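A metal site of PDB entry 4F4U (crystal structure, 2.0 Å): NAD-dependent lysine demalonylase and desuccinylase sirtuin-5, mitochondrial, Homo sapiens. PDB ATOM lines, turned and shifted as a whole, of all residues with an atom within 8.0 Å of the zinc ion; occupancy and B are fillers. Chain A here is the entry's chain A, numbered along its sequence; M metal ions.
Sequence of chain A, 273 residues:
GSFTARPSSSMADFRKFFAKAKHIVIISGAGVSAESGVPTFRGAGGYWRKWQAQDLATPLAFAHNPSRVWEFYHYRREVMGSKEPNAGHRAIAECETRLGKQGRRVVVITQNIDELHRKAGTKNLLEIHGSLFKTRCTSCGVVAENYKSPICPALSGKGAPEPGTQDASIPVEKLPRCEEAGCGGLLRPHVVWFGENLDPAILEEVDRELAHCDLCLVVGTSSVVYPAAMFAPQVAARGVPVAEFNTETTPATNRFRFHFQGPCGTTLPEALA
Within 4 Å of the zinc ion: Cys 137, Cys 140, Cys 178 and Cys 183.
The zinc ion is bound by SG of Cys 140 (2.1 Å), SG of Cys 183 (2.3 Å), SG of Cys 178 (2.4 Å) and SG of Cys 137 (2.5 Å).
The side-chain sulfur of Cys 140 forms a disulfide with the side-chain sulfur of Cys 137 (2.4 Å). N of Gly 185 sits close to SG of Cys 183. N of Cys 178 lies within hydrogen-bond range of O of Gly 185 (2.9 Å). O of Cys 178 is in hydrogen-bond range of N of Gly 184, 3.4 Å away. The backbone NH (N) of Glu 180 lies close to the side-chain sulfur (SG) of Cys 178, at 3.4 Å. N of Cys 137 is in hydrogen-bond range of O of Val 142 (3.1 Å). N of Ser 139 lies close to SG of Cys 137 (3.5 Å).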
ATOM      1  N   ARG A 136      13.845  -6.919  -6.369  1.00  0.00           N
ATOM      2  CA  ARG A 136      13.048  -7.597  -5.353  1.00  0.00           C
ATOM      3  C   ARG A 136      12.296  -8.755  -6.018  1.00  0.00           C
ATOM      4  O   ARG A 136      11.707  -8.598  -7.095  1.00  0.00           O
ATOM      5  CB  ARG A 136      12.063  -6.619  -4.680  1.00  0.00           C
ATOM      6  CG  ARG A 136      11.159  -7.292  -3.651  1.00  0.00           C
ATOM      7  CD  ARG A 136      10.437  -6.294  -2.743  1.00  0.00           C
ATOM      8  NE  ARG A 136       9.221  -5.747  -3.337  1.00  0.00           N
ATOM      9  CZ  ARG A 136       9.069  -4.459  -3.646  1.00  0.00           C
ATOM     10  NH1 ARG A 136      10.059  -3.606  -3.436  1.00  0.00           N
ATOM     11  NH2 ARG A 136       7.936  -4.042  -4.171  1.00  0.00           N
ATOM     12  N   CYS A 137      12.346  -9.926  -5.398  1.00  0.00           N
ATOM     13  CA  CYS A 137      11.646 -11.078  -5.956  1.00  0.00           C
ATOM     14  C   CYS A 137      10.151 -11.016  -5.638  1.00  0.00           C
ATOM     15  O   CYS A 137       9.768 -10.843  -4.479  1.00  0.00           O
ATOM     16  CB  CYS A 137      12.261 -12.386  -5.426  1.00  0.00           C
ATOM     17  SG  CYS A 137      11.581 -13.927  -6.149  1.00  0.00           S
ATOM     18  N   THR A 138       9.312 -11.137  -6.661  1.00  0.00           N
ATOM     19  CA  THR A 138       7.861 -11.069  -6.487  1.00  0.00           C
ATOM     20  C   THR A 138       7.322 -12.318  -5.772  1.00  0.00           C
ATOM     21  O   THR A 138       6.146 -12.365  -5.365  1.00  0.00           O
ATOM     22  CB  THR A 138       7.144 -10.872  -7.834  1.00  0.00           C
ATOM     23  OG1 THR A 138       7.457 -11.963  -8.703  1.00  0.00           O
ATOM     24  CG2 THR A 138       7.619  -9.588  -8.497  1.00  0.00           C
ATOM     25  N   SER A 139       8.173 -13.328  -5.606  1.00  0.00           N
ATOM     26  CA  SER A 139       7.771 -14.553  -4.902  1.00  0.00           C
ATOM     27  C   SER A 139       8.287 -14.613  -3.439  1.00  0.00           C
ATOM     28  O   SER A 139       7.493 -14.623  -2.499  1.00  0.00           O
ATOM     29  CB  SER A 139       8.232 -15.783  -5.685  1.00  0.00           C
ATOM     30  OG  SER A 139       7.325 -16.864  -5.533  1.00  0.00           O
ATOM     31  N   CYS A 140       9.602 -14.622  -3.273  1.00  0.00           N
ATOM     32  CA  CYS A 140      10.301 -14.737  -1.980  1.00  0.00           C
ATOM     33  C   CYS A 140      10.471 -13.400  -1.266  1.00  0.00           C
ATOM     34  O   CYS A 140      10.785 -13.374  -0.075  1.00  0.00           O
ATOM     35  CB  CYS A 140      11.696 -15.218  -2.288  1.00  0.00           C
ATOM     36  SG  CYS A 140      12.014 -14.515  -3.853  1.00  0.00           S
ATOM     37  N   GLY A 141      10.307 -12.305  -1.984  1.00  0.00           N
ATOM     38  CA  GLY A 141      10.409 -10.969  -1.391  1.00  0.00           C
ATOM     39  C   GLY A 141      11.816 -10.471  -1.113  1.00  0.00           C
ATOM     40  O   GLY A 141      11.981  -9.322  -0.693  1.00  0.00           O
ATOM     41  N   VAL A 142      12.824 -11.312  -1.356  1.00  0.00           N
ATOM     42  CA  VAL A 142      14.213 -10.944  -1.101  1.00  0.00           C
ATOM     43  C   VAL A 142      14.698  -9.735  -1.917  1.00  0.00           C
ATOM     44  O   VAL A 142      14.411  -9.613  -3.116  1.00  0.00           O
ATOM     45  CB  VAL A 142      15.174 -12.149  -1.299  1.00  0.00           C
ATOM     46  CG1 VAL A 142      15.014 -12.752  -2.670  1.00  0.00           C
ATOM     47  CG2 VAL A 142      16.619 -11.758  -1.055  1.00  0.00           C
ATOM     48  N   ARG A 177      15.340 -13.605 -13.155  1.00  0.00           N
ATOM     49  CA  ARG A 177      14.739 -14.546 -12.243  1.00  0.00           C
ATOM     50  C   ARG A 177      15.611 -14.665 -11.006  1.00  0.00           C
ATOM     51  O   ARG A 177      16.826 -14.459 -11.065  1.00  0.00           O
ATOM     52  CB  ARG A 177      14.587 -15.908 -12.918  1.00  0.00           C
ATOM     53  CG  ARG A 177      13.874 -15.874 -14.256  1.00  0.00           C
ATOM     54  CD  ARG A 177      12.473 -15.291 -14.135  1.00  0.00           C
ATOM     55  NE  ARG A 177      11.581 -16.132 -13.332  1.00  0.00           N
ATOM     56  CZ  ARG A 177      10.312 -16.374 -13.625  1.00  0.00           C
ATOM     57  NH1 ARG A 177       9.771 -15.830 -14.708  1.00  0.00           N
ATOM     58  NH2 ARG A 177       9.572 -17.159 -12.844  1.00  0.00           N
ATOM     59  N   CYS A 178      14.980 -14.983  -9.892  1.00  0.00           N
ATOM     60  CA  CYS A 178      15.664 -15.094  -8.614  1.00  0.00           C
ATOM     61  C   CYS A 178      16.609 -16.297  -8.562  1.00  0.00           C
ATOM     62  O   CYS A 178      16.257 -17.376  -9.043  1.00  0.00           O
ATOM     63  CB  CYS A 178      14.623 -15.194  -7.491  1.00  0.00           C
ATOM     64  SG  CYS A 178      15.272 -15.312  -5.834  1.00  0.00           S
ATOM     65  N   GLU A 179      17.793 -16.092  -7.999  1.00  0.00           N
ATOM     66  CA  GLU A 179      18.801 -17.141  -7.905  1.00  0.00           C
ATOM     67  C   GLU A 179      19.008 -17.584  -6.453  1.00  0.00           C
ATOM     68  O   GLU A 179      20.019 -18.195  -6.122  1.00  0.00           O
ATOM     69  CB  GLU A 179      20.130 -16.672  -8.508  1.00  0.00           C
ATOM     70  CG  GLU A 179      20.046 -16.301  -9.985  1.00  0.00           C
ATOM     71  CD  GLU A 179      21.370 -15.884 -10.595  1.00  0.00           C
ATOM     72  OE1 GLU A 179      22.284 -15.474  -9.842  1.00  0.00           O
ATOM     73  OE2 GLU A 179      21.509 -15.950 -11.828  1.00  0.00           O
ATOM     74  N   GLU A 180      18.030 -17.278  -5.610  1.00  0.00           N
ATOM     75  CA  GLU A 180      18.130 -17.563  -4.175  1.00  0.00           C
ATOM     76  C   GLU A 180      17.378 -18.831  -3.780  1.00  0.00           C
ATOM     77  O   GLU A 180      16.156 -18.896  -3.921  1.00  0.00           O
ATOM     78  CB  GLU A 180      17.583 -16.383  -3.371  1.00  0.00           C
ATOM     79  CG  GLU A 180      17.715 -16.537  -1.868  1.00  0.00           C
ATOM     80  CD  GLU A 180      19.126 -16.273  -1.384  1.00  0.00           C
ATOM     81  OE1 GLU A 180      19.889 -15.616  -2.118  1.00  0.00           O
ATOM     82  OE2 GLU A 180      19.461 -16.719  -0.259  1.00  0.00           O
ATOM     83  N   ALA A 181      18.114 -19.819  -3.282  1.00  0.00           N
ATOM     84  CA  ALA A 181      17.532 -21.089  -2.815  1.00  0.00           C
ATOM     85  C   ALA A 181      16.681 -21.781  -3.863  1.00  0.00           C
ATOM     86  O   ALA A 181      15.691 -22.444  -3.536  1.00  0.00           O
ATOM     87  CB  ALA A 181      16.741 -20.880  -1.535  1.00  0.00           C
ATOM     88  N   GLY A 182      17.065 -21.618  -5.128  1.00  0.00           N
ATOM     89  CA  GLY A 182      16.330 -22.198  -6.234  1.00  0.00           C
ATOM     90  C   GLY A 182      14.912 -21.677  -6.346  1.00  0.00           C
ATOM     91  O   GLY A 182      14.014 -22.417  -6.744  1.00  0.00           O
ATOM     92  N   CYS A 183      14.699 -20.396  -6.012  1.00  0.00           N
ATOM     93  CA  CYS A 183      13.357 -19.816  -6.047  1.00  0.00           C
ATOM     94  C   CYS A 183      12.745 -19.763  -7.445  1.00  0.00           C
ATOM     95  O   CYS A 183      11.673 -20.328  -7.690  1.00  0.00           O
ATOM     96  CB  CYS A 183      13.353 -18.416  -5.429  1.00  0.00           C
ATOM     97  SG  CYS A 183      11.716 -17.617  -5.469  1.00  0.00           S
ATOM     98  N   GLY A 184      13.415 -19.075  -8.370  1.00  0.00           N
ATOM     99  CA  GLY A 184      12.965 -19.037  -9.750  1.00  0.00           C
ATOM    100  C   GLY A 184      11.898 -17.988  -9.994  1.00  0.00           C
ATOM    101  O   GLY A 184      11.386 -17.850 -11.118  1.00  0.00           O
ATOM    102  N   GLY A 185      11.570 -17.240  -8.955  1.00  0.00           N
ATOM    103  CA  GLY A 185      10.557 -16.201  -9.040  1.00  0.00           C
ATOM    104  C   GLY A 185      10.928 -15.049  -9.942  1.00  0.00           C
ATOM    105  O   GLY A 185      12.115 -14.759 -10.163  1.00  0.00           O
ATOM    106  N   LEU A 186       9.916 -14.385 -10.480  1.00  0.00           N
ATOM    107  CA  LEU A 186      10.107 -13.218 -11.327  1.00  0.00           C
ATOM    108  C   LEU A 186      10.592 -12.023 -10.505  1.00  0.00           C
ATOM    109  O   LEU A 186       9.966 -11.622  -9.509  1.00  0.00           O
ATOM    110  CB  LEU A 186       8.805 -12.875 -12.049  1.00  0.00           C
ATOM    111  CG  LEU A 186       8.825 -11.575 -12.874  1.00  0.00           C
ATOM    112  CD1 LEU A 186       9.701 -11.740 -14.088  1.00  0.00           C
ATOM    113  CD2 LEU A 186       7.406 -11.191 -13.288  1.00  0.00           C
ATOM    114  N   LEU A 187      11.728 -11.457 -10.909  1.00  0.00           N
ATOM    115  CA  LEU A 187      12.262 -10.304 -10.224  1.00  0.00           C
ATOM    116  C   LEU A 187      11.624  -9.035 -10.755  1.00  0.00           C
ATOM    117  O   LEU A 187      11.214  -8.975 -11.923  1.00  0.00           O
ATOM    118  CB  LEU A 187      13.786 -10.219 -10.398  1.00  0.00           C
ATOM    119  CG  LEU A 187      14.639 -11.307  -9.764  1.00  0.00           C
ATOM    120  CD1 LEU A 187      16.123 -10.949  -9.850  1.00  0.00           C
ATOM    121  CD2 LEU A 187      14.227 -11.478  -8.326  1.00  0.00           C
HETATM  122 ZN    ZN M   1      13.019 -15.728  -5.293  1.00  0.00          ZN
